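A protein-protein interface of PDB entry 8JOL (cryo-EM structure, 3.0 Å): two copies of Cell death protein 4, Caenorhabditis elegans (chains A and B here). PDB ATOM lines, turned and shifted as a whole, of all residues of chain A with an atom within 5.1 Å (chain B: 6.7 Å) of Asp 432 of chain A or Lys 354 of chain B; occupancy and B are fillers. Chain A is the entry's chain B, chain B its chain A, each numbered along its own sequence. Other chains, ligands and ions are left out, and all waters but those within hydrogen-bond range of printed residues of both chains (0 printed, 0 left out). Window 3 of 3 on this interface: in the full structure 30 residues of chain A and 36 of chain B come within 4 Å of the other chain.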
ATOM      1  N   ASP A 428     -11.415 -10.144  -7.420  1.00  0.00           N
ATOM      2  CA  ASP A 428     -11.695 -10.068  -8.843  1.00  0.00           C
ATOM      3  C   ASP A 428     -12.556 -11.270  -9.156  1.00  0.00           C
ATOM      4  O   ASP A 428     -13.318 -11.267 -10.111  1.00  0.00           O
ATOM      5  CB  ASP A 428     -10.404 -10.162  -9.659  1.00  0.00           C
ATOM      6  CG  ASP A 428      -9.378  -9.100  -9.284  1.00  0.00           C
ATOM      7  OD1 ASP A 428      -8.598  -9.326  -8.327  1.00  0.00           O
ATOM      8  OD2 ASP A 428      -9.337  -8.045  -9.961  1.00  0.00           O
ATOM      9  N   GLU A 429     -12.421 -12.301  -8.332  1.00  0.00           N
ATOM     10  CA  GLU A 429     -13.243 -13.487  -8.443  1.00  0.00           C
ATOM     11  C   GLU A 429     -14.714 -13.128  -8.562  1.00  0.00           C
ATOM     12  O   GLU A 429     -15.470 -13.821  -9.234  1.00  0.00           O
ATOM     13  CB  GLU A 429     -13.059 -14.365  -7.219  1.00  0.00           C
ATOM     14  CG  GLU A 429     -13.899 -15.624  -7.242  1.00  0.00           C
ATOM     15  CD  GLU A 429     -13.184 -16.780  -7.909  1.00  0.00           C
ATOM     16  OE1 GLU A 429     -12.262 -16.527  -8.723  1.00  0.00           O
ATOM     17  OE2 GLU A 429     -13.543 -17.943  -7.614  1.00  0.00           O
ATOM     18  N   VAL A 430     -15.127 -12.045  -7.917  1.00  0.00           N
ATOM     19  CA  VAL A 430     -16.493 -11.561  -8.084  1.00  0.00           C
ATOM     20  C   VAL A 430     -16.760 -11.222  -9.562  1.00  0.00           C
ATOM     21  O   VAL A 430     -17.739 -11.675 -10.164  1.00  0.00           O
ATOM     22  CB  VAL A 430     -16.762 -10.330  -7.203  1.00  0.00           C
ATOM     23  CG1 VAL A 430     -18.249 -10.076  -7.075  1.00  0.00           C
ATOM     24  CG2 VAL A 430     -16.177 -10.544  -5.853  1.00  0.00           C
ATOM     25  N   ALA A 431     -15.872 -10.436 -10.155  1.00  0.00           N
ATOM     26  CA  ALA A 431     -16.017 -10.080 -11.553  1.00  0.00           C
ATOM     27  C   ALA A 431     -16.088 -11.308 -12.468  1.00  0.00           C
ATOM     28  O   ALA A 431     -16.886 -11.332 -13.396  1.00  0.00           O
ATOM     29  CB  ALA A 431     -14.895  -9.159 -11.974  1.00  0.00           C
ATOM     30  N   ASP A 432     -15.268 -12.326 -12.207  1.00  0.00           N
ATOM     31  CA  ASP A 432     -15.246 -13.530 -13.048  1.00  0.00           C
ATOM     32  C   ASP A 432     -16.588 -14.228 -13.059  1.00  0.00           C
ATOM     33  O   ASP A 432     -17.021 -14.768 -14.078  1.00  0.00           O
ATOM     34  CB  ASP A 432     -14.201 -14.524 -12.553  1.00  0.00           C
ATOM     35  CG  ASP A 432     -12.836 -13.912 -12.438  1.00  0.00           C
ATOM     36  OD1 ASP A 432     -12.689 -12.713 -12.763  1.00  0.00           O
ATOM     37  OD2 ASP A 432     -11.909 -14.634 -12.018  1.00  0.00           O
ATOM     38  N   ARG A 433     -17.224 -14.247 -11.899  1.00  0.00           N
ATOM     39  CA  ARG A 433     -18.525 -14.867 -11.776  1.00  0.00           C
ATOM     40  C   ARG A 433     -19.547 -14.038 -12.528  1.00  0.00           C
ATOM     41  O   ARG A 433     -20.369 -14.572 -13.266  1.00  0.00           O
ATOM     42  CB  ARG A 433     -18.914 -15.019 -10.304  1.00  0.00           C
ATOM     43  CG  ARG A 433     -18.429 -16.303  -9.661  1.00  0.00           C
ATOM     44  CD  ARG A 433     -18.731 -16.326  -8.165  1.00  0.00           C
ATOM     45  NE  ARG A 433     -18.511 -17.642  -7.560  1.00  0.00           N
ATOM     46  CZ  ARG A 433     -17.314 -18.205  -7.380  1.00  0.00           C
ATOM     47  NH1 ARG A 433     -16.211 -17.574  -7.764  1.00  0.00           N
ATOM     48  NH2 ARG A 433     -17.214 -19.407  -6.822  1.00  0.00           N
ATOM     49  N   LEU A 434     -19.471 -12.722 -12.368  1.00  0.00           N
ATOM     50  CA  LEU A 434     -20.423 -11.819 -13.019  1.00  0.00           C
ATOM     51  C   LEU A 434     -20.318 -11.790 -14.565  1.00  0.00           C
ATOM     52  O   LEU A 434     -21.302 -11.512 -15.269  1.00  0.00           O
ATOM     53  CB  LEU A 434     -20.289 -10.413 -12.438  1.00  0.00           C
ATOM     54  CG  LEU A 434     -20.569 -10.322 -10.941  1.00  0.00           C
ATOM     55  CD1 LEU A 434     -20.665  -8.873 -10.475  1.00  0.00           C
ATOM     56  CD2 LEU A 434     -21.847 -11.054 -10.665  1.00  0.00           C
ATOM     57  N   LYS A 435     -19.138 -12.095 -15.098  1.00  0.00           N
ATOM     58  CA  LYS A 435     -19.020 -12.292 -16.536  1.00  0.00           C
ATOM     59  C   LYS A 435     -19.722 -13.577 -16.952  1.00  0.00           C
ATOM     60  O   LYS A 435     -20.664 -13.519 -17.740  1.00  0.00           O
ATOM     61  CB  LYS A 435     -17.566 -12.268 -17.003  1.00  0.00           C
ATOM     62  CG  LYS A 435     -17.021 -10.847 -17.242  1.00  0.00           C
ATOM     63  CD  LYS A 435     -17.799 -10.061 -18.333  1.00  0.00           C
ATOM     64  CE  LYS A 435     -17.046  -8.766 -18.763  1.00  0.00           C
ATOM     65  NZ  LYS A 435     -17.867  -7.719 -19.454  1.00  0.00           N
ATOM     66  N   ARG A 436     -19.301 -14.720 -16.402  1.00  0.00           N
ATOM     67  CA  ARG A 436     -19.998 -16.001 -16.641  1.00  0.00           C
ATOM     68  C   ARG A 436     -21.521 -15.786 -16.592  1.00  0.00           C
ATOM     69  O   ARG A 436     -22.290 -16.390 -17.327  1.00  0.00           O
ATOM     70  CB  ARG A 436     -19.567 -17.074 -15.617  1.00  0.00           C
ATOM     71  CG  ARG A 436     -18.655 -18.199 -16.155  1.00  0.00           C
ATOM     72  CD  ARG A 436     -18.253 -19.179 -15.061  1.00  0.00           C
ATOM     73  NE  ARG A 436     -17.527 -18.493 -13.983  1.00  0.00           N
ATOM     74  CZ  ARG A 436     -17.256 -19.000 -12.771  1.00  0.00           C
ATOM     75  NH1 ARG A 436     -16.583 -18.277 -11.873  1.00  0.00           N
ATOM     76  NH2 ARG A 436     -17.648 -20.228 -12.441  1.00  0.00           N
ATOM     77  N   GLU B 341     -10.422 -13.470 -20.778  1.00  0.00           N
ATOM     78  CA  GLU B 341     -11.350 -12.669 -21.568  1.00  0.00           C
ATOM     79  C   GLU B 341     -10.955 -11.187 -21.678  1.00  0.00           C
ATOM     80  O   GLU B 341     -11.083 -10.594 -22.750  1.00  0.00           O
ATOM     81  CB  GLU B 341     -12.766 -12.816 -21.003  1.00  0.00           C
ATOM     82  CG  GLU B 341     -13.696 -11.670 -21.345  1.00  0.00           C
ATOM     83  CD  GLU B 341     -13.820 -10.678 -20.209  1.00  0.00           C
ATOM     84  OE1 GLU B 341     -14.218  -9.524 -20.467  1.00  0.00           O
ATOM     85  OE2 GLU B 341     -13.513 -11.054 -19.058  1.00  0.00           O
ATOM     86  N   LYS B 347      -5.167  -9.099 -16.245  1.00  0.00           N
ATOM     87  CA  LYS B 347      -6.010 -10.273 -16.006  1.00  0.00           C
ATOM     88  C   LYS B 347      -5.310 -11.566 -16.424  1.00  0.00           C
ATOM     89  O   LYS B 347      -5.726 -12.658 -16.052  1.00  0.00           O
ATOM     90  CB  LYS B 347      -7.356 -10.143 -16.729  1.00  0.00           C
ATOM     91  CG  LYS B 347      -8.517 -10.856 -16.030  1.00  0.00           C
ATOM     92  CD  LYS B 347      -8.544 -12.354 -16.326  1.00  0.00           C
ATOM     93  CE  LYS B 347      -9.647 -13.073 -15.537  1.00  0.00           C
ATOM     94  NZ  LYS B 347      -9.319 -13.246 -14.089  1.00  0.00           N
ATOM     95  N   ALA B 349      -2.094 -11.957 -15.659  1.00  0.00           N
ATOM     96  CA  ALA B 349      -1.328 -12.208 -14.445  1.00  0.00           C
ATOM     97  C   ALA B 349      -2.199 -12.639 -13.244  1.00  0.00           C
ATOM     98  O   ALA B 349      -1.738 -13.386 -12.377  1.00  0.00           O
ATOM     99  CB  ALA B 349      -0.483 -10.997 -14.096  1.00  0.00           C
ATOM    100  N   GLN B 350      -3.445 -12.168 -13.194  1.00  0.00           N
ATOM    101  CA  GLN B 350      -4.401 -12.620 -12.184  1.00  0.00           C
ATOM    102  C   GLN B 350      -4.465 -14.129 -12.203  1.00  0.00           C
ATOM    103  O   GLN B 350      -4.427 -14.789 -11.163  1.00  0.00           O
ATOM    104  CB  GLN B 350      -5.809 -12.135 -12.512  1.00  0.00           C
ATOM    105  CG  GLN B 350      -6.203 -10.791 -11.957  1.00  0.00           C
ATOM    106  CD  GLN B 350      -7.695 -10.536 -12.132  1.00  0.00           C
ATOM    107  OE1 GLN B 350      -8.505 -11.471 -12.076  1.00  0.00           O
ATOM    108  NE2 GLN B 350      -8.066  -9.271 -12.352  1.00  0.00           N
ATOM    109  N   LEU B 351      -4.599 -14.657 -13.411  1.00  0.00           N
ATOM    110  CA  LEU B 351      -4.715 -16.084 -13.637  1.00  0.00           C
ATOM    111  C   LEU B 351      -3.421 -16.799 -13.253  1.00  0.00           C
ATOM    112  O   LEU B 351      -3.457 -17.881 -12.671  1.00  0.00           O
ATOM    113  CB  LEU B 351      -5.063 -16.356 -15.106  1.00  0.00           C
ATOM    114  CG  LEU B 351      -6.296 -15.650 -15.681  1.00  0.00           C
ATOM    115  CD1 LEU B 351      -6.855 -16.468 -16.830  1.00  0.00           C
ATOM    116  CD2 LEU B 351      -7.351 -15.423 -14.593  1.00  0.00           C
ATOM    117  N   ASN B 352      -2.281 -16.193 -13.577  1.00  0.00           N
ATOM    118  CA  ASN B 352      -0.996 -16.781 -13.236  1.00  0.00           C
ATOM    119  C   ASN B 352      -0.945 -17.118 -11.749  1.00  0.00           C
ATOM    120  O   ASN B 352      -0.272 -18.061 -11.335  1.00  0.00           O
ATOM    121  CB  ASN B 352       0.152 -15.841 -13.604  1.00  0.00           C
ATOM    122  CG  ASN B 352       0.586 -15.976 -15.060  1.00  0.00           C
ATOM    123  OD1 ASN B 352       0.748 -17.081 -15.580  1.00  0.00           O
ATOM    124  ND2 ASN B 352       0.799 -14.840 -15.715  1.00  0.00           N
ATOM    125  N   ASN B 353      -1.672 -16.339 -10.956  1.00  0.00           N
ATOM    126  CA  ASN B 353      -1.832 -16.595  -9.525  1.00  0.00           C
ATOM    127  C   ASN B 353      -2.773 -17.767  -9.262  1.00  0.00           C
ATOM    128  O   ASN B 353      -2.371 -18.781  -8.667  1.00  0.00           O
ATOM    129  CB  ASN B 353      -2.379 -15.349  -8.827  1.00  0.00           C
ATOM    130  CG  ASN B 353      -1.505 -14.126  -9.046  1.00  0.00           C
ATOM    131  OD1 ASN B 353      -0.343 -14.241  -9.456  1.00  0.00           O
ATOM    132  ND2 ASN B 353      -2.060 -12.948  -8.773  1.00  0.00           N
ATOM    133  N   LYS B 354      -4.017 -17.605  -9.726  1.00  0.00           N
ATOM    134  CA  LYS B 354      -5.073 -18.616  -9.622  1.00  0.00           C
ATOM    135  C   LYS B 354      -4.523 -20.013  -9.884  1.00  0.00           C
ATOM    136  O   LYS B 354      -5.049 -21.013  -9.381  1.00  0.00           O
ATOM    137  CB  LYS B 354      -6.176 -18.311 -10.643  1.00  0.00           C
ATOM    138  CG  LYS B 354      -7.611 -18.536 -10.155  1.00  0.00           C
ATOM    139  CD  LYS B 354      -8.597 -18.343 -11.310  1.00  0.00           C
ATOM    140  CE  LYS B 354      -9.971 -17.848 -10.853  1.00  0.00           C
ATOM    141  NZ  LYS B 354     -10.564 -18.684  -9.786  1.00  0.00           N
ATOM    142  N   LEU B 355      -3.470 -20.074 -10.696  1.00  0.00           N
ATOM    143  CA  LEU B 355      -2.860 -21.344 -11.087  1.00  0.00           C
ATOM    144  C   LEU B 355      -2.012 -21.957  -9.975  1.00  0.00           C
ATOM    145  O   LEU B 355      -1.931 -23.180  -9.861  1.00  0.00           O
ATOM    146  CB  LEU B 355      -2.046 -21.186 -12.382  1.00  0.00           C
ATOM    147  CG  LEU B 355      -2.531 -21.881 -13.668  1.00  0.00           C
ATOM    148  CD1 LEU B 355      -2.467 -23.391 -13.518  1.00  0.00           C
ATOM    149  CD2 LEU B 355      -3.925 -21.444 -14.109  1.00  0.00           C
ATOM    150  N   GLU B 356      -1.390 -21.107  -9.160  1.00  0.00           N
ATOM    151  CA  GLU B 356      -0.570 -21.571  -8.043  1.00  0.00           C
ATOM    152  C   GLU B 356      -1.418 -21.935  -6.815  1.00  0.00           C
ATOM    153  O   GLU B 356      -1.097 -22.865  -6.057  1.00  0.00           O
ATOM    154  CB  GLU B 356       0.480 -20.517  -7.699  1.00  0.00           C
ATOM    155  CG  GLU B 356       1.523 -20.323  -8.801  1.00  0.00           C
ATOM    156  CD  GLU B 356       2.212 -18.963  -8.752  1.00  0.00           C
ATOM    157  OE1 GLU B 356       2.243 -18.340  -7.664  1.00  0.00           O
ATOM    158  OE2 GLU B 356       2.723 -18.511  -9.806  1.00  0.00           O
ATOM    159  N   SER B 357      -2.514 -21.209  -6.640  1.00  0.00           N
ATOM    160  CA  SER B 357      -3.402 -21.434  -5.506  1.00  0.00           C
ATOM    161  C   SER B 357      -4.717 -22.161  -5.840  1.00  0.00           C
ATOM    162  O   SER B 357      -5.697 -22.045  -5.098  1.00  0.00           O
ATOM    163  CB  SER B 357      -3.723 -20.102  -4.827  1.00  0.00           C
ATOM    164  OG  SER B 357      -4.686 -19.356  -5.564  1.00  0.00           O
ATOM    165  N   ARG B 358      -4.758 -22.894  -6.950  1.00  0.00           N
ATOM    166  CA  ARG B 358      -5.946 -23.683  -7.298  1.00  0.00           C
ATOM    167  C   ARG B 358      -5.626 -24.764  -8.327  1.00  0.00           C
ATOM    168  O   ARG B 358      -6.530 -25.463  -8.809  1.00  0.00           O
ATOM    169  CB  ARG B 358      -7.080 -22.793  -7.841  1.00  0.00           C
ATOM    170  CG  ARG B 358      -8.104 -22.310  -6.810  1.00  0.00           C
ATOM    171  CD  ARG B 358      -9.493 -22.208  -7.435  1.00  0.00           C
ATOM    172  NE  ARG B 358     -10.316 -21.181  -6.799  1.00  0.00           N
ATOM    173  CZ  ARG B 358     -11.646 -21.191  -6.783  1.00  0.00           C
ATOM    174  NH1 ARG B 358     -12.311 -22.188  -7.364  1.00  0.00           N
ATOM    175  NH2 ARG B 358     -12.310 -20.209  -6.179  1.00  0.00           N
ATOM    176  N   GLY B 359      -4.348 -24.888  -8.687  1.00  0.00           N
ATOM    177  CA  GLY B 359      -3.928 -25.864  -9.684  1.00  0.00           C
ATOM    178  C   GLY B 359      -4.637 -25.625 -11.007  1.00  0.00           C
ATOM    179  O   GLY B 359      -5.121 -24.518 -11.284  1.00  0.00           O
ATOM    180  N   LEU B 360      -4.719 -26.657 -11.835  1.00  0.00           N
ATOM    181  CA  LEU B 360      -5.314 -26.500 -13.155  1.00  0.00           C
ATOM    182  C   LEU B 360      -6.784 -26.083 -13.083  1.00  0.00           C
ATOM    183  O   LEU B 360      -7.342 -25.668 -14.084  1.00  0.00           O
ATOM    184  CB  LEU B 360      -5.159 -27.784 -13.980  1.00  0.00           C
ATOM    185  CG  LEU B 360      -3.763 -28.258 -14.430  1.00  0.00           C
ATOM    186  CD1 LEU B 360      -2.639 -27.372 -13.913  1.00  0.00           C
ATOM    187  CD2 LEU B 360      -3.506 -29.705 -14.046  1.00  0.00           C
ATOM    188  N   VAL B 361      -7.403 -26.198 -11.906  1.00  0.00           N
ATOM    189  CA  VAL B 361      -8.845 -25.968 -11.744  1.00  0.00           C
ATOM    190  C   VAL B 361      -9.168 -24.481 -11.749  1.00  0.00           C
ATOM    191  O   VAL B 361     -10.331 -24.074 -11.667  1.00  0.00           O
ATOM    192  CB  VAL B 361      -9.393 -26.604 -10.431  1.00  0.00           C
ATOM    193  CG1 VAL B 361     -10.897 -26.830 -10.532  1.00  0.00           C
ATOM    194  CG2 VAL B 361      -8.677 -27.916 -10.108  1.00  0.00           C
ATOM    195  N   GLY B 362      -8.121 -23.675 -11.833  1.00  0.00           N
ATOM    196  CA  GLY B 362      -8.282 -22.242 -11.768  1.00  0.00           C
ATOM    197  C   GLY B 362      -8.604 -21.685 -13.130  1.00  0.00           C
ATOM    198  O   GLY B 362      -9.106 -20.571 -13.270  1.00  0.00           O
ATOM    199  N   VAL B 363      -8.331 -22.493 -14.145  1.00  0.00           N
ATOM    200  CA  VAL B 363      -8.460 -22.090 -15.543  1.00  0.00           C
ATOM    201  C   VAL B 363      -9.284 -23.115 -16.356  1.00  0.00           C
ATOM    202  O   VAL B 363      -9.450 -22.983 -17.558  1.00  0.00           O
ATOM    203  CB  VAL B 363      -7.060 -21.889 -16.154  1.00  0.00           C
ATOM    204  CG1 VAL B 363      -6.678 -23.083 -17.029  1.00  0.00           C
ATOM    205  CG2 VAL B 363      -6.983 -20.558 -16.884  1.00  0.00           C
ATOM    206  N   HIS B 466      -2.260 -30.848  -6.164  1.00  0.00           N
ATOM    207  CA  HIS B 466      -3.639 -30.655  -5.708  1.00  0.00           C
ATOM    208  C   HIS B 466      -4.433 -31.961  -5.555  1.00  0.00           C
ATOM    209  O   HIS B 466      -5.455 -31.997  -4.855  1.00  0.00           O
ATOM    210  CB  HIS B 466      -4.351 -29.673  -6.641  1.00  0.00           C
ATOM    211  CG  HIS B 466      -3.722 -28.315  -6.662  1.00  0.00           C
ATOM    212  ND1 HIS B 466      -2.526 -28.059  -7.298  1.00  0.00           N
ATOM    213  CD2 HIS B 466      -4.113 -27.142  -6.111  1.00  0.00           C
ATOM    214  CE1 HIS B 466      -2.210 -26.786  -7.143  1.00  0.00           C
ATOM    215  NE2 HIS B 466      -3.157 -26.207  -6.426  1.00  0.00           N
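Among the printed residues, merely in contact across the chains: Asp 432 of chain A with Lys 354 of chain B (3.9 Å) and Lys 435 of chain A with Glu 341 of chain B (3.4 Å).
Of the 18 printed residues of chain B, 5 touch a printed residue of chain A.
Of the 9 printed residues of chain A, 4 touch a printed residue of chain B.
Among the printed residues, 6 pairs touch across the chains.
Among the printed residues, Asp or Glu carboxylates within 4 Å of a Lys or Arg side-chain nitrogen of the other chain: Glu 429 of chain A with Lys 354 of chain B (2.9 Å), Glu 429 of chain A with Arg 358 of chain B (3.0 Å) and Asp 432 of chain A with Lys 347 of chain B (3.6 Å).
The side-chain carboxylate (OD2) of Asp 432 of chain A lies within salt-bridge range of the side-chain amino group (NZ) of Lys 347 of chain B.
NE2 of Gln 350 of chain B lies within hydrogen-bond range of OD2 of Asp 428 of chain A (3.0 Å).
The side-chain amino group (NZ) of Lys 354 of chain B lies within salt-bridge range of the side-chain carboxylate (OE1) of Glu 429 of chain A.
The side-chain carboxylate (OE2) of Glu 429 of chain A is in salt-bridge range of the guanidinium group (NH2) of Arg 358 of chain B (3.0 Å).
Of chain A, only Glu 429 (2.9 Å) and Asp 432 (3.9 Å) come within 4 Å of Lys 354 of chain B.
Printed residues of chain B within 4 Å of Asp 428 of chain A: Gln 350.
Of the printed residues of chain A, Lys 347 of chain B touches Asp 432.
Of the printed residues of chain B, Lys 435 of chain A touches Glu 341.
Gly 362 of chain B touches none of the printed residues of chain A.
Leu 351 of chain B touches none of the printed residues of chain A.
The nearest residue of chain B that does not touch Asp 432 of chain A is Gln 350 of chain B (4.4 Å).
The nearest printed residue of chain A that does not touch Lys 347 of chain B is Asp 428 of chain A (5.5 Å).
The side-chain amino group (NZ) of Lys 347 of chain B sits at hydrogen-bond distance from the side-chain amide oxygen (OE1) of Gln 350 of chain B, at 2.8 Å.
The side-chain carboxylate of Glu 429 of chain A lies within salt-bridge range of the guanidinium group of Arg 433 of chain A.
No position is printed for both chains.
Of the 6 pairs that touch across the chains among the printed residues, none has its exchanged pair printed and touching as well.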
